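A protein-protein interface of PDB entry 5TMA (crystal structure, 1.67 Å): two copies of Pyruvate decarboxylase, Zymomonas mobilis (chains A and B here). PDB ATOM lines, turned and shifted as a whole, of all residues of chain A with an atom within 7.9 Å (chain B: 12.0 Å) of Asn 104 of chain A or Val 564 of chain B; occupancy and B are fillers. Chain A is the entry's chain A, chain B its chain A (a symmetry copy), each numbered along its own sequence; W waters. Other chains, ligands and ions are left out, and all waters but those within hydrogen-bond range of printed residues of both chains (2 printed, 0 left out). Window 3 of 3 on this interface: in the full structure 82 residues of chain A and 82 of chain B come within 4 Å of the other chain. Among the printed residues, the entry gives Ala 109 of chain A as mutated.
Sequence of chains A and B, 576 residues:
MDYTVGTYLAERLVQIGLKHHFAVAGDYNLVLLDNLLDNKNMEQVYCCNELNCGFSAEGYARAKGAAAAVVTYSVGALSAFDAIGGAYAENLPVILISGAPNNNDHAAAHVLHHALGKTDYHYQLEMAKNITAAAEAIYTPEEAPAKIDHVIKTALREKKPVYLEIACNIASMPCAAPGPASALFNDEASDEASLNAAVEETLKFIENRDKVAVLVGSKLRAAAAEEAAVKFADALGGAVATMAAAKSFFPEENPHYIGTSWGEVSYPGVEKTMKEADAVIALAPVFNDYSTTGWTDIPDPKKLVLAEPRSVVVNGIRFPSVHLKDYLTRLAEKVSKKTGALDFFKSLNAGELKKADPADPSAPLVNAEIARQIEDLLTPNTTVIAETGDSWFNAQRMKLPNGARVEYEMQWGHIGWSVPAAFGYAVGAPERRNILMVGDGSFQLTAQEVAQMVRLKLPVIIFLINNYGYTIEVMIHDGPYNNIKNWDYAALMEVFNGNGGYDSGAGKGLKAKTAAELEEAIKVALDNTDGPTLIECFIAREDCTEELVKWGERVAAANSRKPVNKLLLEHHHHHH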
ATOM      1  N   PRO A 101      27.161  -0.687   5.897  1.00  0.00           N
ATOM      2  CA  PRO A 101      26.155  -0.425   6.906  1.00  0.00           C
ATOM      3  C   PRO A 101      24.726  -0.507   6.380  1.00  0.00           C
ATOM      4  O   PRO A 101      24.449  -0.327   5.159  1.00  0.00           O
ATOM      5  CB  PRO A 101      26.424   1.018   7.291  1.00  0.00           C
ATOM      6  CG  PRO A 101      27.958   1.179   7.194  1.00  0.00           C
ATOM      7  CD  PRO A 101      28.217   0.361   5.932  1.00  0.00           C
ATOM      8  N   ASN A 102      23.844  -0.734   7.347  1.00  0.00           N
ATOM      9  CA  ASN A 102      22.388  -0.659   7.163  1.00  0.00           C
ATOM     10  C   ASN A 102      22.091   0.633   6.468  1.00  0.00           C
ATOM     11  O   ASN A 102      22.608   1.679   6.856  1.00  0.00           O
ATOM     12  CB  ASN A 102      21.704  -0.775   8.543  1.00  0.00           C
ATOM     13  CG  ASN A 102      20.205  -0.848   8.435  1.00  0.00           C
ATOM     14  OD1 ASN A 102      19.601   0.154   8.105  1.00  0.00           O
ATOM     15  ND2 ASN A 102      19.623  -2.036   8.665  1.00  0.00           N
ATOM     16  N   ASN A 103      21.270   0.589   5.426  1.00  0.00           N
ATOM     17  CA  ASN A 103      21.050   1.792   4.641  1.00  0.00           C
ATOM     18  C   ASN A 103      20.351   2.950   5.376  1.00  0.00           C
ATOM     19  O   ASN A 103      20.533   4.118   4.983  1.00  0.00           O
ATOM     20  CB  ASN A 103      20.388   1.554   3.314  1.00  0.00           C
ATOM     21  CG  ASN A 103      18.898   1.113   3.382  1.00  0.00           C
ATOM     22  OD1 ASN A 103      18.298   1.008   4.441  1.00  0.00           O
ATOM     23  ND2 ASN A 103      18.347   0.742   2.195  1.00  0.00           N
ATOM     24  N   ASN A 104      19.756   2.636   6.519  1.00  0.00           N
ATOM     25  CA  ASN A 104      19.182   3.656   7.390  1.00  0.00           C
ATOM     26  C   ASN A 104      20.260   4.466   8.151  1.00  0.00           C
ATOM     27  O   ASN A 104      19.912   5.501   8.741  1.00  0.00           O
ATOM     28  CB  ASN A 104      18.226   3.034   8.427  1.00  0.00           C
ATOM     29  CG  ASN A 104      17.007   2.389   7.803  1.00  0.00           C
ATOM     30  OD1 ASN A 104      16.246   3.047   7.098  1.00  0.00           O
ATOM     31  ND2 ASN A 104      16.881   1.077   7.979  1.00  0.00           N
ATOM     32  N   ASP A 105      21.527   3.998   8.190  1.00  0.00           N
ATOM     33  CA  ASP A 105      22.550   4.599   9.026  1.00  0.00           C
ATOM     34  C   ASP A 105      23.305   5.751   8.342  1.00  0.00           C
ATOM     35  O   ASP A 105      24.027   6.500   8.976  1.00  0.00           O
ATOM     36  CB  ASP A 105      23.513   3.524   9.523  1.00  0.00           C
ATOM     37  CG  ASP A 105      22.910   2.670  10.646  1.00  0.00           C
ATOM     38  OD1 ASP A 105      22.155   3.210  11.522  1.00  0.00           O
ATOM     39  OD2 ASP A 105      23.234   1.487  10.712  1.00  0.00           O
ATOM     40  N   HIS A 106      23.084   5.927   7.063  1.00  0.00           N
ATOM     41  CA  HIS A 106      23.639   7.074   6.302  1.00  0.00           C
ATOM     42  C   HIS A 106      22.914   8.368   6.686  1.00  0.00           C
ATOM     43  O   HIS A 106      21.692   8.430   6.788  1.00  0.00           O
ATOM     44  CB  HIS A 106      23.519   6.856   4.783  1.00  0.00           C
ATOM     45  CG  HIS A 106      24.311   5.698   4.307  1.00  0.00           C
ATOM     46  ND1 HIS A 106      25.664   5.792   4.083  1.00  0.00           N
ATOM     47  CD2 HIS A 106      23.992   4.393   4.143  1.00  0.00           C
ATOM     48  CE1 HIS A 106      26.158   4.588   3.834  1.00  0.00           C
ATOM     49  NE2 HIS A 106      25.165   3.722   3.852  1.00  0.00           N
ATOM     50  N   ALA A 107      23.711   9.410   6.837  1.00  0.00           N
ATOM     51  CA  ALA A 107      23.266  10.724   7.185  1.00  0.00           C
ATOM     52  C   ALA A 107      22.311  10.719   8.350  1.00  0.00           C
ATOM     53  O   ALA A 107      21.278  11.372   8.339  1.00  0.00           O
ATOM     54  CB  ALA A 107      22.633  11.383   5.929  1.00  0.00           C
ATOM     55  N   ALA A 108      22.655   9.981   9.396  1.00  0.00           N
ATOM     56  CA  ALA A 108      21.788   9.779  10.503  1.00  0.00           C
ATOM     57  C   ALA A 108      22.514  10.091  11.808  1.00  0.00           C
ATOM     58  O   ALA A 108      22.011   9.777  12.837  1.00  0.00           O
ATOM     59  CB  ALA A 108      21.311   8.335  10.518  1.00  0.00           C
ATOM     60  N   ALA A 109      23.729  10.622  11.753  1.00  0.00           N
ATOM     61  CA  ALA A 109      24.563  10.820  12.993  1.00  0.00           C
ATOM     62  C   ALA A 109      24.731   9.548  13.832  1.00  0.00           C
ATOM     63  O   ALA A 109      24.784   9.592  15.064  1.00  0.00           O
ATOM     64  CB  ALA A 109      23.977  11.930  13.892  1.00  0.00           C
ATOM     65  N   HIS A 110      24.820   8.422  13.167  1.00  0.00           N
ATOM     66  CA  HIS A 110      25.067   7.148  13.845  1.00  0.00           C
ATOM     67  C   HIS A 110      26.555   6.726  13.746  1.00  0.00           C
ATOM     68  O   HIS A 110      27.102   6.596  12.657  1.00  0.00           O
ATOM     69  CB  HIS A 110      24.200   6.063  13.224  1.00  0.00           C
ATOM     70  CG  HIS A 110      22.771   6.157  13.583  1.00  0.00           C
ATOM     71  ND1 HIS A 110      21.781   5.470  12.891  1.00  0.00           N
ATOM     72  CD2 HIS A 110      22.134   6.932  14.495  1.00  0.00           C
ATOM     73  CE1 HIS A 110      20.612   5.778  13.410  1.00  0.00           C
ATOM     74  NE2 HIS A 110      20.798   6.652  14.385  1.00  0.00           N
ATOM     75  N   LEU A 112      29.039   3.731  14.083  1.00  0.00           N
ATOM     76  CA  LEU A 112      28.910   2.293  13.866  1.00  0.00           C
ATOM     77  C   LEU A 112      30.230   1.545  14.101  1.00  0.00           C
ATOM     78  O   LEU A 112      31.371   2.053  13.854  1.00  0.00           O
ATOM     79  CB  LEU A 112      28.429   1.953  12.445  1.00  0.00           C
ATOM     80  CG  LEU A 112      27.068   2.454  12.051  1.00  0.00           C
ATOM     81  CD1 LEU A 112      26.858   2.088  10.590  1.00  0.00           C
ATOM     82  CD2 LEU A 112      26.067   1.751  12.985  1.00  0.00           C
ATOM     83  N   TYR A 139      23.036   1.070  -2.200  1.00  0.00           N
ATOM     84  CA  TYR A 139      22.322   1.417  -1.027  1.00  0.00           C
ATOM     85  C   TYR A 139      20.843   0.925  -1.050  1.00  0.00           C
ATOM     86  O   TYR A 139      20.227   0.832   0.037  1.00  0.00           O
ATOM     87  CB  TYR A 139      22.311   2.915  -0.813  1.00  0.00           C
ATOM     88  CG  TYR A 139      23.648   3.540  -0.744  1.00  0.00           C
ATOM     89  CD1 TYR A 139      24.575   3.218   0.255  1.00  0.00           C
ATOM     90  CD2 TYR A 139      24.000   4.433  -1.697  1.00  0.00           C
ATOM     91  CE1 TYR A 139      25.835   3.867   0.266  1.00  0.00           C
ATOM     92  CE2 TYR A 139      25.241   5.025  -1.728  1.00  0.00           C
ATOM     93  CZ  TYR A 139      26.136   4.789  -0.754  1.00  0.00           C
ATOM     94  OH  TYR A 139      27.394   5.416  -0.791  1.00  0.00           O
ATOM     95  N   ALA A 167      24.701  -2.559   1.064  1.00  0.00           N
ATOM     96  CA  ALA A 167      24.143  -2.353   2.372  1.00  0.00           C
ATOM     97  C   ALA A 167      23.695  -3.644   2.979  1.00  0.00           C
ATOM     98  O   ALA A 167      23.079  -4.473   2.297  1.00  0.00           O
ATOM     99  CB  ALA A 167      22.966  -1.336   2.285  1.00  0.00           C
ATOM    100  N   ASN A 169      21.331  -4.600   4.812  1.00  0.00           N
ATOM    101  CA  ASN A 169      19.889  -4.885   4.996  1.00  0.00           C
ATOM    102  C   ASN A 169      19.150  -4.959   3.698  1.00  0.00           C
ATOM    103  O   ASN A 169      17.894  -5.013   3.726  1.00  0.00           O
ATOM    104  CB  ASN A 169      19.212  -3.859   5.912  1.00  0.00           C
ATOM    105  CG  ASN A 169      19.294  -2.454   5.401  1.00  0.00           C
ATOM    106  OD1 ASN A 169      20.267  -2.076   4.784  1.00  0.00           O
ATOM    107  ND2 ASN A 169      18.317  -1.628   5.752  1.00  0.00           N
ATOM    108  N   ILE A 170      19.853  -5.062   2.556  1.00  0.00           N
ATOM    109  CA  ILE A 170      19.170  -5.196   1.287  1.00  0.00           C
ATOM    110  C   ILE A 170      19.555  -6.411   0.432  1.00  0.00           C
ATOM    111  O   ILE A 170      19.007  -6.590  -0.645  1.00  0.00           O
ATOM    112  CB  ILE A 170      19.385  -3.997   0.406  1.00  0.00           C
ATOM    113  CG1 ILE A 170      20.858  -3.882  -0.049  1.00  0.00           C
ATOM    114  CG2 ILE A 170      18.855  -2.762   1.110  1.00  0.00           C
ATOM    115  CD1 ILE A 170      21.040  -2.758  -1.011  1.00  0.00           C
ATOM    116  N   ASP B 289      26.435   1.456  17.780  1.00  0.00           N
ATOM    117  CA  ASP B 289      25.508   0.314  17.718  1.00  0.00           C
ATOM    118  C   ASP B 289      25.799  -0.811  18.698  1.00  0.00           C
ATOM    119  O   ASP B 289      24.860  -1.477  19.182  1.00  0.00           O
ATOM    120  CB  ASP B 289      25.337  -0.193  16.285  1.00  0.00           C
ATOM    121  CG  ASP B 289      26.602  -0.692  15.653  1.00  0.00           C
ATOM    122  OD1 ASP B 289      27.703  -0.133  15.934  1.00  0.00           O
ATOM    123  OD2 ASP B 289      26.488  -1.654  14.862  1.00  0.00           O
ATOM    124  N   GLY B 294      22.714  -2.708  20.192  1.00  0.00           N
ATOM    125  CA  GLY B 294      21.860  -2.604  19.004  1.00  0.00           C
ATOM    126  C   GLY B 294      20.837  -1.489  19.032  1.00  0.00           C
ATOM    127  O   GLY B 294      19.718  -1.678  18.579  1.00  0.00           O
ATOM    128  N   TRP B 295      21.226  -0.352  19.585  1.00  0.00           N
ATOM    129  CA  TRP B 295      20.385   0.833  19.738  1.00  0.00           C
ATOM    130  C   TRP B 295      19.185   0.630  20.723  1.00  0.00           C
ATOM    131  O   TRP B 295      18.267   1.401  20.667  1.00  0.00           O
ATOM    132  CB  TRP B 295      19.845   1.438  18.437  1.00  0.00           C
ATOM    133  CG  TRP B 295      20.881   1.682  17.376  1.00  0.00           C
ATOM    134  CD1 TRP B 295      20.923   1.091  16.171  1.00  0.00           C
ATOM    135  CD2 TRP B 295      21.983   2.630  17.406  1.00  0.00           C
ATOM    136  NE1 TRP B 295      22.011   1.551  15.452  1.00  0.00           N
ATOM    137  CE2 TRP B 295      22.676   2.492  16.181  1.00  0.00           C
ATOM    138  CE3 TRP B 295      22.475   3.524  18.359  1.00  0.00           C
ATOM    139  CZ2 TRP B 295      23.845   3.208  15.874  1.00  0.00           C
ATOM    140  CZ3 TRP B 295      23.712   4.225  18.064  1.00  0.00           C
ATOM    141  CH2 TRP B 295      24.358   4.054  16.820  1.00  0.00           C
ATOM    142  N   VAL B 555      22.002  -7.129  18.238  1.00  0.00           N
ATOM    143  CA  VAL B 555      22.887  -6.671  17.121  1.00  0.00           C
ATOM    144  C   VAL B 555      22.386  -7.210  15.764  1.00  0.00           C
ATOM    145  O   VAL B 555      22.346  -6.479  14.783  1.00  0.00           O
ATOM    146  CB  VAL B 555      24.388  -7.071  17.428  1.00  0.00           C
ATOM    147  CG1 VAL B 555      25.257  -7.299  16.169  1.00  0.00           C
ATOM    148  CG2 VAL B 555      24.944  -6.038  18.404  1.00  0.00           C
ATOM    149  N   ALA B 556      22.023  -8.477  15.696  1.00  0.00           N
ATOM    150  CA  ALA B 556      21.543  -9.003  14.459  1.00  0.00           C
ATOM    151  C   ALA B 556      20.274  -8.124  14.085  1.00  0.00           C
ATOM    152  O   ALA B 556      20.118  -7.709  12.918  1.00  0.00           O
ATOM    153  CB  ALA B 556      21.205 -10.464  14.609  1.00  0.00           C
ATOM    154  N   ALA B 557      19.434  -7.790  15.073  1.00  0.00           N
ATOM    155  CA  ALA B 557      18.188  -7.004  14.799  1.00  0.00           C
ATOM    156  C   ALA B 557      18.436  -5.637  14.319  1.00  0.00           C
ATOM    157  O   ALA B 557      17.749  -5.179  13.399  1.00  0.00           O
ATOM    158  CB  ALA B 557      17.228  -6.952  15.990  1.00  0.00           C
ATOM    159  N   ALA B 558      19.403  -4.955  14.902  1.00  0.00           N
ATOM    160  CA  ALA B 558      19.720  -3.618  14.410  1.00  0.00           C
ATOM    161  C   ALA B 558      20.281  -3.678  12.985  1.00  0.00           C
ATOM    162  O   ALA B 558      19.879  -2.904  12.160  1.00  0.00           O
ATOM    163  CB  ALA B 558      20.713  -2.902  15.301  1.00  0.00           C
ATOM    164  N   ASN B 559      21.172  -4.629  12.700  1.00  0.00           N
ATOM    165  CA  ASN B 559      21.833  -4.675  11.383  1.00  0.00           C
ATOM    166  C   ASN B 559      20.848  -4.933  10.293  1.00  0.00           C
ATOM    167  O   ASN B 559      20.991  -4.388   9.167  1.00  0.00           O
ATOM    168  CB  ASN B 559      22.909  -5.819  11.340  1.00  0.00           C
ATOM    169  CG  ASN B 559      24.122  -5.512  12.261  1.00  0.00           C
ATOM    170  OD1 ASN B 559      24.276  -4.380  12.798  1.00  0.00           O
ATOM    171  ND2 ASN B 559      24.973  -6.556  12.481  1.00  0.00           N
ATOM    172  N   SER B 560      19.879  -5.819  10.588  1.00  0.00           N
ATOM    173  CA  SER B 560      18.964  -6.244   9.548  1.00  0.00           C
ATOM    174  C   SER B 560      17.728  -5.391   9.466  1.00  0.00           C
ATOM    175  O   SER B 560      16.842  -5.704   8.636  1.00  0.00           O
ATOM    176  CB  SER B 560      18.536  -7.703   9.756  1.00  0.00           C
ATOM    177  OG  SER B 560      17.795  -7.841  10.945  1.00  0.00           O
ATOM    178  N   ARG B 561      17.568  -4.387  10.296  1.00  0.00           N
ATOM    179  CA  ARG B 561      16.313  -3.643  10.218  1.00  0.00           C
ATOM    180  C   ARG B 561      15.993  -3.089   8.833  1.00  0.00           C
ATOM    181  O   ARG B 561      16.861  -2.574   8.127  1.00  0.00           O
ATOM    182  CB  ARG B 561      16.238  -2.549  11.288  1.00  0.00           C
ATOM    183  CG  ARG B 561      16.965  -1.267  10.984  1.00  0.00           C
ATOM    184  CD  ARG B 561      17.070  -0.455  12.241  1.00  0.00           C
ATOM    185  NE  ARG B 561      17.763   0.808  12.062  1.00  0.00           N
ATOM    186  CZ  ARG B 561      19.097   0.946  12.055  1.00  0.00           C
ATOM    187  NH1 ARG B 561      19.895  -0.079  12.264  1.00  0.00           N
ATOM    188  NH2 ARG B 561      19.608   2.167  11.949  1.00  0.00           N
ATOM    189  N   LYS B 562      14.711  -3.162   8.433  1.00  0.00           N
ATOM    190  CA  LYS B 562      14.276  -2.834   7.068  1.00  0.00           C
ATOM    191  C   LYS B 562      14.539  -1.417   6.734  1.00  0.00           C
ATOM    192  O   LYS B 562      14.494  -0.572   7.637  1.00  0.00           O
ATOM    193  CB  LYS B 562      12.697  -3.094   6.839  1.00  0.00           C
ATOM    194  N   PRO B 563      14.757  -1.103   5.439  1.00  0.00           N
ATOM    195  CA  PRO B 563      14.773   0.268   5.001  1.00  0.00           C
ATOM    196  C   PRO B 563      13.447   0.988   5.331  1.00  0.00           C
ATOM    197  O   PRO B 563      12.399   0.389   5.163  1.00  0.00           O
ATOM    198  CB  PRO B 563      14.913   0.182   3.462  1.00  0.00           C
ATOM    199  CG  PRO B 563      15.453  -1.184   3.170  1.00  0.00           C
ATOM    200  CD  PRO B 563      14.970  -2.050   4.322  1.00  0.00           C
ATOM    201  N   VAL B 564      13.533   2.245   5.771  1.00  0.00           N
ATOM    202  CA  VAL B 564      12.346   3.114   5.981  1.00  0.00           C
ATOM    203  C   VAL B 564      11.940   3.867   4.693  1.00  0.00           C
ATOM    204  O   VAL B 564      12.746   4.008   3.757  1.00  0.00           O
ATOM    205  CB  VAL B 564      12.621   4.102   7.147  1.00  0.00           C
ATOM    206  CG1 VAL B 564      13.070   3.340   8.403  1.00  0.00           C
ATOM    207  CG2 VAL B 564      13.658   5.164   6.725  1.00  0.00           C
ATOM    208  N   ASN B 565      10.717   4.380   4.621  1.00  0.00           N
ATOM    209  CA  ASN B 565      10.337   5.217   3.460  1.00  0.00           C
ATOM    210  C   ASN B 565      11.076   6.603   3.296  1.00  0.00           C
ATOM    211  O   ASN B 565      11.107   7.412   4.226  1.00  0.00           O
ATOM    212  CB  ASN B 565       8.838   5.481   3.400  1.00  0.00           C
ATOM    213  CG  ASN B 565       8.429   5.978   2.021  1.00  0.00           C
ATOM    214  OD1 ASN B 565       8.352   7.195   1.763  1.00  0.00           O
ATOM    215  ND2 ASN B 565       8.287   5.033   1.090  1.00  0.00           N
ATOM    216  N   LYS B 566      11.638   6.829   2.103  1.00  0.00           N
ATOM    217  CA  LYS B 566      12.462   8.006   1.764  1.00  0.00           C
ATOM    218  C   LYS B 566      11.747   9.092   0.898  1.00  0.00           C
ATOM    219  O   LYS B 566      12.410  10.088   0.524  1.00  0.00           O
ATOM    220  CB  LYS B 566      13.751   7.536   1.041  1.00  0.00           C
ATOM    221  CG  LYS B 566      14.757   6.722   1.869  1.00  0.00           C
ATOM    222  CD  LYS B 566      15.037   7.360   3.234  1.00  0.00           C
ATOM    223  CE  LYS B 566      16.475   7.187   3.707  1.00  0.00           C
ATOM    224  NZ  LYS B 566      17.349   8.175   3.042  1.00  0.00           N
ATOM    225  N   LEU B 567      10.455   8.878   0.559  1.00  0.00           N
ATOM    226  CA  LEU B 567       9.614   9.834  -0.214  1.00  0.00           C
ATOM    227  C   LEU B 567       8.268   9.941   0.508  1.00  0.00           C
ATOM    228  O   LEU B 567       8.029  10.867   1.280  1.00  0.00           O
ATOM    229  CB  LEU B 567       9.312   9.359  -1.646  1.00  0.00           C
ATOM    230  CG  LEU B 567      10.388   9.098  -2.706  1.00  0.00           C
ATOM    231  CD1 LEU B 567       9.960   8.107  -3.793  1.00  0.00           C
ATOM    232  CD2 LEU B 567      10.841  10.403  -3.343  1.00  0.00           C
HETATM  233  O   HOH W   1      16.046  -5.601   5.694  1.00  0.00           O
HETATM  234  O   HOH W   2      22.598   0.229  12.949  1.00  0.00           O
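ND2 of Asn 102 of chain A lies within hydrogen-bond range of O of Asn 559 of chain B (2.8 Å).
The side-chain amide nitrogen (ND2) of Asn 102 of chain A is in hydrogen-bond range of the backbone carbonyl oxygen (O) of Arg 561 of chain B (2.9 Å).
ND2 of Asn 104 of chain A is in hydrogen-bond range of O of Lys 562 of chain B, 2.9 Å away.
The backbone NH (N) of Val 564 of chain B lies within hydrogen-bond range of the side-chain amide oxygen (OD1) of Asn 104 of chain A (3.1 Å).
The guanidinium group of Arg 561 of chain B is in salt-bridge range of the side-chain carboxylate of Asp 105 of chain A.
ND2 of Asn 169 of chain A is in hydrogen-bond range of O of Arg 561 of chain B (2.9 Å).
ND2 of Asn 169 of chain A lies close to ND2 of Asn 102 of chain A.
The backbone NH (N) of Asn 103 of chain A lies within hydrogen-bond range of the side-chain amide oxygen (OD1) of Asn 169 of chain A (2.9 Å).
OD1 of Asp 105 of chain A lies within hydrogen-bond range of ND1 of His 110 of chain A, at 2.7 Å.
The backbone carbonyl oxygen (O) of Val 555 of chain B sits close to the side-chain amide oxygen (OD1) of Asn 559 of chain B (3.5 Å).
The side-chain hydroxyl of Ser 560 of chain B is in hydrogen-bond range of the backbone carbonyl oxygen of Ala 556 of chain B, 3.1 Å away.
The backbone carbonyl oxygen of Ala 558 of chain B sits at hydrogen-bond distance from the guanidinium group of Arg 561 of chain B, at 2.8 Å.
Among the printed residues, pairs that only touch across the chains: Leu 112 of chain A with Asp 289 of chain B, Asn 102 of chain A with Ala 558 of chain B, Asn 103 of chain A with Pro 563 of chain B, Asn 169 of chain A with Pro 563 of chain B, Asn 104 of chain A with Arg 561 of chain B, Asn 104 of chain A with Pro 563 of chain B, Asn 169 of chain A with Asn 559 of chain B, His 110 of chain A with Trp 295 of chain B, Asn 169 of chain A with Lys 562 of chain B, Leu 112 of chain A with Trp 295 of chain B and Asn 102 of chain A with Ser 560 of chain B.
Asn 103 of chain A touches just one residue of chain B: Pro 563 (3.6 Å).
Of the printed residues of chain B, Asn 104 of chain A touches Arg 561 (3.7 Å), Lys 562 (2.9 Å), Pro 563 (3.7 Å) and Val 564 (3.1 Å).
No residue of chain B comes within 4 Å of Ala 107 of chain A.
No residue of chain B comes within 4 Å of Ala 108 of chain A.
Printed residues of chain B within 4 Å of Leu 112 of chain A: Asp 289 and Trp 295.
Of the printed residues of chain A, Asn 559 of chain B touches Asn 102 and Asn 169.
Val 564 of chain B touches just one residue of chain A: Asn 104.
The nearest printed residue of chain B that does not touch Leu 112 of chain A is Asn 559 of chain B (6.4 Å).
Hydrophobic or aromatic side chains of chain A that line the printed part of chain B: His 110 and Leu 112.
Of the 16 printed residues of chain B, 9 touch a printed residue of chain A.
Printed residues of chain B that touch a printed residue of chain A: Asp 289, Trp 295, Ala 558, Asn 559, Ser 560, Arg 561, Lys 562, Pro 563 and Val 564.
Along chain B the printed residues that touch a printed residue of chain A span positions 289 to 564.
Among the printed residues, Asp or Glu carboxylates within 4 Å of a Lys or Arg side-chain nitrogen of the other chain: Asp 105 of chain A with Arg 561 of chain B (2.8 Å).
No position is printed for both chains.
Of the 17 pairs that touch across the chains among the printed residues, none has its exchanged pair printed and touching as well.
Water W2 lies within hydrogen-bond range of OD2 of Asp 105 of chain A, NH1 of Arg 561 of chain B and NE1 of Trp 295 of chain B.
Water W1 lies within hydrogen-bond range of O of Asn 169 of chain A and O of Ser 560 of chain B.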
